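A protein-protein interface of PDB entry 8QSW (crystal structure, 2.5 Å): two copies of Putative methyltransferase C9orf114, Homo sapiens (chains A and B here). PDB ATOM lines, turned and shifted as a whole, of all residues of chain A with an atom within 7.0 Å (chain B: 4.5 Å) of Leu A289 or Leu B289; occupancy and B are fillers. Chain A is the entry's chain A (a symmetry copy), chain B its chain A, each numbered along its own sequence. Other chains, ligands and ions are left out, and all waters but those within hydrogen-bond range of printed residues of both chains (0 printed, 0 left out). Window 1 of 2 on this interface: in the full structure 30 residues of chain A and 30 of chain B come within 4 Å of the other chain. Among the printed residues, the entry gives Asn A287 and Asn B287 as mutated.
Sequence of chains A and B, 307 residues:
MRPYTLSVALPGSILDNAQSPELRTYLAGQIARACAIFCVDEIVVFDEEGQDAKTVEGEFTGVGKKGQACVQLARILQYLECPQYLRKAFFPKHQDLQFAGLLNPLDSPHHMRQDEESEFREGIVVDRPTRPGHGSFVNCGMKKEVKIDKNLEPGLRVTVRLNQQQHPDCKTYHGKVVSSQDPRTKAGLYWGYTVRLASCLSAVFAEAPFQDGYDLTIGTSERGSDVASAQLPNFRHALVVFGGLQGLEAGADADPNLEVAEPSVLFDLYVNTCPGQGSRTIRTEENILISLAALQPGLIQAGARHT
Printed residues of chain B that touch a printed residue of chain A: Glu B286, Leu B289, Ile B290 and Ala B293.
Hydrophobic or aromatic side chains of chain B within 4 Å of the printed part of chain A: Leu B289 and Ala B293.
Of the 21 printed residues of chain A, 5 touch a printed residue of chain B.
Hydrophobic or aromatic side chains of chain A that line the printed part of chain B: Ile A37, Leu A289 and Ala A293.
Along chain A the printed residues that touch a printed residue of chain B span positions 33 to 293.
Among the printed residues, Asp or Glu carboxylates within 4 Å of a Lys or Arg side-chain nitrogen of the other chain: Arg A33 with Glu B286.
Ile A37 touches Glu B286 (CD1 to OE1, 3.8 Å).
Leu A289 touches Leu B289 (CD1 to CD1, 3.8 Å).
Ile A290 touches Ala B293.
Ala A293 touches Ile B290.
Ala A293 touches Ala B293.
Leu A289 touches its own counterpart, Leu B289.
Ile A290 touches Ala B293, and with the chains exchanged Ala A293 touches Ile B290.
Ala A293 touches its own counterpart, Ala B293.
Of the 6 pairs that touch across the chains among the printed residues, 4 have their exchanged pair printed and touching as well.
Leu A289 touches just one residue of chain B: Leu B289.
Of chain A, only Leu A289 (3.8 Å) comes within 4 Å of Leu B289.
Of the printed residues of chain B, Ala A293 touches Ile B290 (3.9 Å) and Ala B293 (3.8 Å).
Of the printed residues of chain B, Arg A33 touches Glu B286 (2.6 Å).
Printed residues of chain A within 4 Å of Ile B290: Ala A293.
Printed residues of chain A within 4 Å of Glu B286: Arg A33 (2.6 Å) and Ile A37 (3.8 Å).
Phe A38 touches none of the printed residues of chain B.
The nearest residue of chain B that does not touch Leu A289 is Glu B286 (4.1 Å).
The nearest residue of chain A that does not touch Leu B289 is Glu A286 (4.1 Å).
OE1 of Glu B286 lies within salt-bridge range of NH1 of Arg A33 (2.6 Å).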
ATOM      1  N   GLN A  30      11.694   8.557  36.255  1.00  0.00           N
ATOM      2  CA  GLN A  30      11.394   7.952  34.949  1.00  0.00           C
ATOM      3  C   GLN A  30      11.101   6.471  35.125  1.00  0.00           C
ATOM      4  O   GLN A  30      10.196   5.933  34.492  1.00  0.00           O
ATOM      5  CB  GLN A  30      12.524   8.104  33.934  1.00  0.00           C
ATOM      6  CG  GLN A  30      13.020   9.541  33.768  1.00  0.00           C
ATOM      7  CD  GLN A  30      14.044   9.631  32.669  1.00  0.00           C
ATOM      8  OE1 GLN A  30      13.752   9.285  31.536  1.00  0.00           O
ATOM      9  NE2 GLN A  30      15.239  10.109  32.974  1.00  0.00           N
ATOM     10  N   ILE A  31      11.801   5.812  36.060  1.00  0.00           N
ATOM     11  CA  ILE A  31      11.542   4.387  36.264  1.00  0.00           C
ATOM     12  C   ILE A  31      10.102   4.165  36.741  1.00  0.00           C
ATOM     13  O   ILE A  31       9.377   3.277  36.273  1.00  0.00           O
ATOM     14  CB  ILE A  31      12.521   3.829  37.302  1.00  0.00           C
ATOM     15  CG1 ILE A  31      13.974   4.131  36.944  1.00  0.00           C
ATOM     16  CG2 ILE A  31      12.263   2.344  37.529  1.00  0.00           C
ATOM     17  CD1 ILE A  31      14.403   3.526  35.642  1.00  0.00           C
ATOM     18  N   ARG A  33       7.538   5.957  36.461  1.00  0.00           N
ATOM     19  CA  ARG A  33       6.522   6.239  35.461  1.00  0.00           C
ATOM     20  C   ARG A  33       6.473   5.069  34.494  1.00  0.00           C
ATOM     21  O   ARG A  33       5.378   4.604  34.150  1.00  0.00           O
ATOM     22  CB  ARG A  33       6.724   7.585  34.772  1.00  0.00           C
ATOM     23  CG  ARG A  33       6.359   8.757  35.659  1.00  0.00           C
ATOM     24  CD  ARG A  33       5.952   9.920  34.765  1.00  0.00           C
ATOM     25  NE  ARG A  33       4.517  10.105  34.812  1.00  0.00           N
ATOM     26  CZ  ARG A  33       3.682   9.862  33.828  1.00  0.00           C
ATOM     27  NH1 ARG A  33       4.130   9.672  32.616  1.00  0.00           N
ATOM     28  NH2 ARG A  33       2.388   9.862  34.063  1.00  0.00           N
ATOM     29  N   ALA A  34       7.648   4.536  34.132  1.00  0.00           N
ATOM     30  CA  ALA A  34       7.614   3.495  33.117  1.00  0.00           C
ATOM     31  C   ALA A  34       6.837   2.323  33.670  1.00  0.00           C
ATOM     32  O   ALA A  34       6.041   1.748  32.946  1.00  0.00           O
ATOM     33  CB  ALA A  34       8.964   3.081  32.629  1.00  0.00           C
ATOM     34  N   CYS A  35       7.036   2.035  34.959  1.00  0.00           N
ATOM     35  CA  CYS A  35       6.451   0.838  35.543  1.00  0.00           C
ATOM     36  C   CYS A  35       4.952   1.045  35.754  1.00  0.00           C
ATOM     37  O   CYS A  35       4.174   0.113  35.581  1.00  0.00           O
ATOM     38  CB  CYS A  35       7.175   0.469  36.833  1.00  0.00           C
ATOM     39  SG  CYS A  35       8.861  -0.149  36.541  1.00  0.00           S
ATOM     40  N   ILE A  37       3.019   2.985  33.883  1.00  0.00           N
ATOM     41  CA  ILE A  37       2.271   3.096  32.647  1.00  0.00           C
ATOM     42  C   ILE A  37       1.828   1.696  32.262  1.00  0.00           C
ATOM     43  O   ILE A  37       0.705   1.481  31.797  1.00  0.00           O
ATOM     44  CB  ILE A  37       3.113   3.759  31.546  1.00  0.00           C
ATOM     45  CG1 ILE A  37       3.318   5.237  31.846  1.00  0.00           C
ATOM     46  CG2 ILE A  37       2.509   3.563  30.146  1.00  0.00           C
ATOM     47  CD1 ILE A  37       4.484   5.802  31.086  1.00  0.00           C
ATOM     48  N   PHE A  38       2.726   0.756  32.513  1.00  0.00           N
ATOM     49  CA  PHE A  38       2.510  -0.612  32.088  1.00  0.00           C
ATOM     50  C   PHE A  38       1.864  -1.424  33.193  1.00  0.00           C
ATOM     51  O   PHE A  38       1.812  -2.622  33.068  1.00  0.00           O
ATOM     52  CB  PHE A  38       3.833  -1.234  31.667  1.00  0.00           C
ATOM     53  CG  PHE A  38       4.202  -0.813  30.284  1.00  0.00           C
ATOM     54  CD1 PHE A  38       3.611  -1.419  29.189  1.00  0.00           C
ATOM     55  CD2 PHE A  38       5.062   0.251  30.076  1.00  0.00           C
ATOM     56  CE1 PHE A  38       3.910  -0.992  27.900  1.00  0.00           C
ATOM     57  CE2 PHE A  38       5.335   0.702  28.787  1.00  0.00           C
ATOM     58  CZ  PHE A  38       4.783   0.060  27.698  1.00  0.00           C
ATOM     59  N   PHE A 242      16.286  -6.236  33.878  1.00  0.00           N
ATOM     60  CA  PHE A 242      17.140  -5.326  33.141  1.00  0.00           C
ATOM     61  C   PHE A 242      18.508  -5.281  33.783  1.00  0.00           C
ATOM     62  O   PHE A 242      18.613  -5.258  35.002  1.00  0.00           O
ATOM     63  CB  PHE A 242      16.545  -3.921  33.099  1.00  0.00           C
ATOM     64  CG  PHE A 242      15.186  -3.947  32.462  1.00  0.00           C
ATOM     65  CD1 PHE A 242      14.055  -4.228  33.222  1.00  0.00           C
ATOM     66  CD2 PHE A 242      15.055  -3.854  31.082  1.00  0.00           C
ATOM     67  CE1 PHE A 242      12.805  -4.274  32.627  1.00  0.00           C
ATOM     68  CE2 PHE A 242      13.809  -3.974  30.480  1.00  0.00           C
ATOM     69  CZ  PHE A 242      12.687  -4.179  31.249  1.00  0.00           C
ATOM     70  N   ARG A 283      19.906   2.929  27.333  1.00  0.00           N
ATOM     71  CA  ARG A 283      19.778   3.154  28.756  1.00  0.00           C
ATOM     72  C   ARG A 283      18.537   2.467  29.290  1.00  0.00           C
ATOM     73  O   ARG A 283      17.572   2.230  28.573  1.00  0.00           O
ATOM     74  CB  ARG A 283      19.772   4.647  29.029  1.00  0.00           C
ATOM     75  CG  ARG A 283      21.030   5.300  28.479  1.00  0.00           C
ATOM     76  CD  ARG A 283      21.815   5.971  29.593  1.00  0.00           C
ATOM     77  NE  ARG A 283      21.002   7.077  30.030  1.00  0.00           N
ATOM     78  CZ  ARG A 283      20.595   8.000  29.191  1.00  0.00           C
ATOM     79  NH1 ARG A 283      21.221   8.131  28.034  1.00  0.00           N
ATOM     80  NH2 ARG A 283      19.615   8.816  29.533  1.00  0.00           N
ATOM     81  N   THR A 284      18.583   2.146  30.577  1.00  0.00           N
ATOM     82  CA  THR A 284      17.659   1.172  31.095  1.00  0.00           C
ATOM     83  C   THR A 284      16.313   1.852  31.300  1.00  0.00           C
ATOM     84  O   THR A 284      15.308   1.197  31.089  1.00  0.00           O
ATOM     85  CB  THR A 284      18.287   0.401  32.264  1.00  0.00           C
ATOM     86  OG1 THR A 284      18.738   1.318  33.242  1.00  0.00           O
ATOM     87  CG2 THR A 284      19.477  -0.425  31.817  1.00  0.00           C
ATOM     88  N   GLU A 285      16.266   3.144  31.639  1.00  0.00           N
ATOM     89  CA  GLU A 285      14.978   3.829  31.629  1.00  0.00           C
ATOM     90  C   GLU A 285      14.390   3.876  30.210  1.00  0.00           C
ATOM     91  O   GLU A 285      13.184   3.784  30.014  1.00  0.00           O
ATOM     92  CB  GLU A 285      15.069   5.228  32.211  1.00  0.00           C
ATOM     93  CG  GLU A 285      15.821   6.254  31.413  1.00  0.00           C
ATOM     94  CD  GLU A 285      17.333   6.287  31.553  1.00  0.00           C
ATOM     95  OE1 GLU A 285      17.918   5.385  32.260  1.00  0.00           O
ATOM     96  OE2 GLU A 285      17.934   7.261  30.968  1.00  0.00           O
ATOM     97  N   GLU A 286      15.248   3.869  29.199  1.00  0.00           N
ATOM     98  CA  GLU A 286      14.805   3.684  27.830  1.00  0.00           C
ATOM     99  C   GLU A 286      14.360   2.245  27.614  1.00  0.00           C
ATOM    100  O   GLU A 286      13.321   1.957  27.017  1.00  0.00           O
ATOM    101  CB  GLU A 286      15.924   4.073  26.863  1.00  0.00           C
ATOM    102  CG  GLU A 286      16.239   5.563  26.923  1.00  0.00           C
ATOM    103  CD  GLU A 286      17.525   6.003  26.248  1.00  0.00           C
ATOM    104  OE1 GLU A 286      18.336   5.087  25.959  1.00  0.00           O
ATOM    105  OE2 GLU A 286      17.724   7.263  26.030  1.00  0.00           O
ATOM    106  N   ASN A 287      15.160   1.325  28.105  1.00  0.00           N
ATOM    107  CA  ASN A 287      14.956  -0.067  27.757  1.00  0.00           C
ATOM    108  C   ASN A 287      13.680  -0.606  28.406  1.00  0.00           C
ATOM    109  O   ASN A 287      12.917  -1.304  27.753  1.00  0.00           O
ATOM    110  CB  ASN A 287      16.236  -0.848  28.031  1.00  0.00           C
ATOM    111  CG  ASN A 287      16.178  -2.223  27.430  1.00  0.00           C
ATOM    112  OD1 ASN A 287      15.499  -2.434  26.426  1.00  0.00           O
ATOM    113  ND2 ASN A 287      16.812  -3.173  28.093  1.00  0.00           N
ATOM    114  N   ILE A 288      13.321  -0.151  29.606  1.00  0.00           N
ATOM    115  CA  ILE A 288      12.039  -0.517  30.219  1.00  0.00           C
ATOM    116  C   ILE A 288      10.852  -0.157  29.312  1.00  0.00           C
ATOM    117  O   ILE A 288       9.942  -0.945  29.118  1.00  0.00           O
ATOM    118  CB  ILE A 288      11.915   0.100  31.626  1.00  0.00           C
ATOM    119  CG1 ILE A 288      13.019  -0.464  32.515  1.00  0.00           C
ATOM    120  CG2 ILE A 288      10.561  -0.155  32.272  1.00  0.00           C
ATOM    121  CD1 ILE A 288      12.946  -0.034  33.957  1.00  0.00           C
ATOM    122  N   LEU A 289      10.815   1.032  28.738  1.00  0.00           N
ATOM    123  CA  LEU A 289       9.658   1.397  27.933  1.00  0.00           C
ATOM    124  C   LEU A 289       9.598   0.544  26.659  1.00  0.00           C
ATOM    125  O   LEU A 289       8.552   0.016  26.279  1.00  0.00           O
ATOM    126  CB  LEU A 289       9.736   2.896  27.613  1.00  0.00           C
ATOM    127  CG  LEU A 289       9.537   3.829  28.803  1.00  0.00           C
ATOM    128  CD1 LEU A 289       9.613   5.286  28.390  1.00  0.00           C
ATOM    129  CD2 LEU A 289       8.193   3.600  29.451  1.00  0.00           C
ATOM    130  N   ILE A 290      10.729   0.430  25.972  1.00  0.00           N
ATOM    131  CA  ILE A 290      10.782  -0.298  24.716  1.00  0.00           C
ATOM    132  C   ILE A 290      10.432  -1.756  25.003  1.00  0.00           C
ATOM    133  O   ILE A 290       9.638  -2.371  24.318  1.00  0.00           O
ATOM    134  CB  ILE A 290      12.187  -0.129  24.096  1.00  0.00           C
ATOM    135  CG1 ILE A 290      12.506   1.331  23.793  1.00  0.00           C
ATOM    136  CG2 ILE A 290      12.388  -0.949  22.852  1.00  0.00           C
ATOM    137  CD1 ILE A 290      13.934   1.554  23.341  1.00  0.00           C
ATOM    138  N   SER A 291      11.013  -2.318  26.055  1.00  0.00           N
ATOM    139  CA  SER A 291      10.923  -3.757  26.265  1.00  0.00           C
ATOM    140  C   SER A 291       9.508  -4.143  26.681  1.00  0.00           C
ATOM    141  O   SER A 291       8.935  -5.087  26.126  1.00  0.00           O
ATOM    142  CB  SER A 291      11.966  -4.218  27.253  1.00  0.00           C
ATOM    143  OG  SER A 291      13.287  -4.215  26.666  1.00  0.00           O
ATOM    144  N   LEU A 292       8.916  -3.353  27.585  1.00  0.00           N
ATOM    145  CA  LEU A 292       7.571  -3.652  28.051  1.00  0.00           C
ATOM    146  C   LEU A 292       6.560  -3.431  26.940  1.00  0.00           C
ATOM    147  O   LEU A 292       5.568  -4.166  26.851  1.00  0.00           O
ATOM    148  CB  LEU A 292       7.211  -2.806  29.265  1.00  0.00           C
ATOM    149  CG  LEU A 292       7.972  -3.214  30.519  1.00  0.00           C
ATOM    150  CD1 LEU A 292       7.376  -2.549  31.744  1.00  0.00           C
ATOM    151  CD2 LEU A 292       7.986  -4.724  30.675  1.00  0.00           C
ATOM    152  N   ALA A 293       6.856  -2.473  26.070  1.00  0.00           N
ATOM    153  CA  ALA A 293       5.983  -2.249  24.935  1.00  0.00           C
ATOM    154  C   ALA A 293       6.062  -3.478  24.035  1.00  0.00           C
ATOM    155  O   ALA A 293       5.035  -4.101  23.716  1.00  0.00           O
ATOM    156  CB  ALA A 293       6.353  -0.960  24.231  1.00  0.00           C
ATOM    157  N   ALA A 294       7.294  -3.859  23.679  1.00  0.00           N
ATOM    158  CA  ALA A 294       7.502  -4.940  22.731  1.00  0.00           C
ATOM    159  C   ALA A 294       6.873  -6.237  23.231  1.00  0.00           C
ATOM    160  O   ALA A 294       6.457  -7.066  22.426  1.00  0.00           O
ATOM    161  CB  ALA A 294       8.975  -5.140  22.466  1.00  0.00           C
ATOM    162  N   LEU A 295       6.838  -6.404  24.554  1.00  0.00           N
ATOM    163  CA  LEU A 295       6.284  -7.584  25.192  1.00  0.00           C
ATOM    164  C   LEU A 295       4.785  -7.514  25.514  1.00  0.00           C
ATOM    165  O   LEU A 295       4.145  -8.550  25.531  1.00  0.00           O
ATOM    166  CB  LEU A 295       7.073  -7.727  26.478  1.00  0.00           C
ATOM    167  CG  LEU A 295       8.468  -8.275  26.264  1.00  0.00           C
ATOM    168  CD1 LEU A 295       9.222  -8.277  27.568  1.00  0.00           C
ATOM    169  CD2 LEU A 295       8.378  -9.658  25.672  1.00  0.00           C
ATOM    170  N   ALA B  34      15.458   8.917  21.470  1.00  0.00           N
ATOM    171  CA  ALA B  34      14.385   7.999  21.125  1.00  0.00           C
ATOM    172  C   ALA B  34      14.392   7.811  19.626  1.00  0.00           C
ATOM    173  O   ALA B  34      14.229   6.689  19.172  1.00  0.00           O
ATOM    174  CB  ALA B  34      13.041   8.425  21.621  1.00  0.00           C
ATOM    175  N   PHE B  38      15.556   4.167  17.163  1.00  0.00           N
ATOM    176  CA  PHE B  38      14.652   3.555  16.211  1.00  0.00           C
ATOM    177  C   PHE B  38      15.040   3.912  14.790  1.00  0.00           C
ATOM    178  O   PHE B  38      14.268   3.652  13.902  1.00  0.00           O
ATOM    179  CB  PHE B  38      13.224   3.992  16.504  1.00  0.00           C
ATOM    180  CG  PHE B  38      12.647   3.203  17.631  1.00  0.00           C
ATOM    181  CD1 PHE B  38      12.171   1.922  17.414  1.00  0.00           C
ATOM    182  CD2 PHE B  38      12.669   3.699  18.923  1.00  0.00           C
ATOM    183  CE1 PHE B  38      11.683   1.163  18.472  1.00  0.00           C
ATOM    184  CE2 PHE B  38      12.214   2.926  19.988  1.00  0.00           C
ATOM    185  CZ  PHE B  38      11.693   1.670  19.758  1.00  0.00           C
ATOM    186  N   GLU B 285       7.938  12.251  25.313  1.00  0.00           N
ATOM    187  CA  GLU B 285       9.195  11.509  25.284  1.00  0.00           C
ATOM    188  C   GLU B 285       8.984  10.052  25.723  1.00  0.00           C
ATOM    189  O   GLU B 285       9.620   9.134  25.217  1.00  0.00           O
ATOM    190  CB  GLU B 285      10.268  12.168  26.132  1.00  0.00           C
ATOM    191  CG  GLU B 285      10.078  12.137  27.621  1.00  0.00           C
ATOM    192  CD  GLU B 285       9.184  13.197  28.241  1.00  0.00           C
ATOM    193  OE1 GLU B 285       8.549  14.011  27.473  1.00  0.00           O
ATOM    194  OE2 GLU B 285       9.153  13.230  29.526  1.00  0.00           O
ATOM    195  N   GLU B 286       7.986   9.810  26.561  1.00  0.00           N
ATOM    196  CA  GLU B 286       7.558   8.456  26.861  1.00  0.00           C
ATOM    197  C   GLU B 286       6.849   7.853  25.657  1.00  0.00           C
ATOM    198  O   GLU B 286       7.078   6.710  25.260  1.00  0.00           O
ATOM    199  CB  GLU B 286       6.659   8.455  28.097  1.00  0.00           C
ATOM    200  CG  GLU B 286       7.417   8.863  29.355  1.00  0.00           C
ATOM    201  CD  GLU B 286       6.569   9.197  30.569  1.00  0.00           C
ATOM    202  OE1 GLU B 286       5.345   9.383  30.350  1.00  0.00           O
ATOM    203  OE2 GLU B 286       7.136   9.291  31.728  1.00  0.00           O
ATOM    204  N   ASN B 287       5.970   8.633  25.069  1.00  0.00           N
ATOM    205  CA  ASN B 287       5.076   8.084  24.069  1.00  0.00           C
ATOM    206  C   ASN B 287       5.844   7.725  22.795  1.00  0.00           C
ATOM    207  O   ASN B 287       5.614   6.667  22.228  1.00  0.00           O
ATOM    208  CB  ASN B 287       3.880   9.013  23.897  1.00  0.00           C
ATOM    209  CG  ASN B 287       2.792   8.364  23.091  1.00  0.00           C
ATOM    210  OD1 ASN B 287       2.660   7.140  23.098  1.00  0.00           O
ATOM    211  ND2 ASN B 287       2.076   9.169  22.328  1.00  0.00           N
ATOM    212  N   ILE B 288       6.884   8.475  22.432  1.00  0.00           N
ATOM    213  CA  ILE B 288       7.749   8.102  21.307  1.00  0.00           C
ATOM    214  C   ILE B 288       8.345   6.698  21.487  1.00  0.00           C
ATOM    215  O   ILE B 288       8.353   5.892  20.574  1.00  0.00           O
ATOM    216  CB  ILE B 288       8.830   9.177  21.076  1.00  0.00           C
ATOM    217  CG1 ILE B 288       8.151  10.494  20.709  1.00  0.00           C
ATOM    218  CG2 ILE B 288       9.825   8.798  19.988  1.00  0.00           C
ATOM    219  CD1 ILE B 288       9.096  11.607  20.340  1.00  0.00           C
ATOM    220  N   LEU B 289       8.865   6.362  22.655  1.00  0.00           N
ATOM    221  CA  LEU B 289       9.489   5.056  22.805  1.00  0.00           C
ATOM    222  C   LEU B 289       8.437   3.943  22.713  1.00  0.00           C
ATOM    223  O   LEU B 289       8.615   2.936  22.026  1.00  0.00           O
ATOM    224  CB  LEU B 289      10.239   5.022  24.144  1.00  0.00           C
ATOM    225  CG  LEU B 289      11.472   5.916  24.224  1.00  0.00           C
ATOM    226  CD1 LEU B 289      12.157   5.806  25.572  1.00  0.00           C
ATOM    227  CD2 LEU B 289      12.478   5.548  23.160  1.00  0.00           C
ATOM    228  N   ILE B 290       7.337   4.110  23.437  1.00  0.00           N
ATOM    229  CA  ILE B 290       6.298   3.096  23.482  1.00  0.00           C
ATOM    230  C   ILE B 290       5.734   2.938  22.072  1.00  0.00           C
ATOM    231  O   ILE B 290       5.562   1.845  21.570  1.00  0.00           O
ATOM    232  CB  ILE B 290       5.227   3.518  24.513  1.00  0.00           C
ATOM    233  CG1 ILE B 290       5.804   3.644  25.918  1.00  0.00           C
ATOM    234  CG2 ILE B 290       4.041   2.595  24.546  1.00  0.00           C
ATOM    235  CD1 ILE B 290       4.826   4.216  26.923  1.00  0.00           C
ATOM    236  N   SER B 291       5.465   4.052  21.404  1.00  0.00           N
ATOM    237  CA  SER B 291       4.712   4.000  20.158  1.00  0.00           C
ATOM    238  C   SER B 291       5.564   3.390  19.050  1.00  0.00           C
ATOM    239  O   SER B 291       5.099   2.500  18.330  1.00  0.00           O
ATOM    240  CB  SER B 291       4.181   5.366  19.798  1.00  0.00           C
ATOM    241  OG  SER B 291       3.075   5.742  20.649  1.00  0.00           O
ATOM    242  N   LEU B 292       6.836   3.803  18.981  1.00  0.00           N
ATOM    243  CA  LEU B 292       7.719   3.285  17.948  1.00  0.00           C
ATOM    244  C   LEU B 292       8.026   1.819  18.193  1.00  0.00           C
ATOM    245  O   LEU B 292       8.166   1.047  17.236  1.00  0.00           O
ATOM    246  CB  LEU B 292       9.011   4.088  17.880  1.00  0.00           C
ATOM    247  CG  LEU B 292       8.812   5.487  17.315  1.00  0.00           C
ATOM    248  CD1 LEU B 292      10.147   6.131  16.999  1.00  0.00           C
ATOM    249  CD2 LEU B 292       7.923   5.451  16.085  1.00  0.00           C
ATOM    250  N   ALA B 293       8.056   1.438  19.465  1.00  0.00           N
ATOM    251  CA  ALA B 293       8.265   0.040  19.784  1.00  0.00           C
ATOM    252  C   ALA B 293       7.050  -0.738  19.289  1.00  0.00           C
ATOM    253  O   ALA B 293       7.183  -1.697  18.508  1.00  0.00           O
ATOM    254  CB  ALA B 293       8.528  -0.129  21.265  1.00  0.00           C
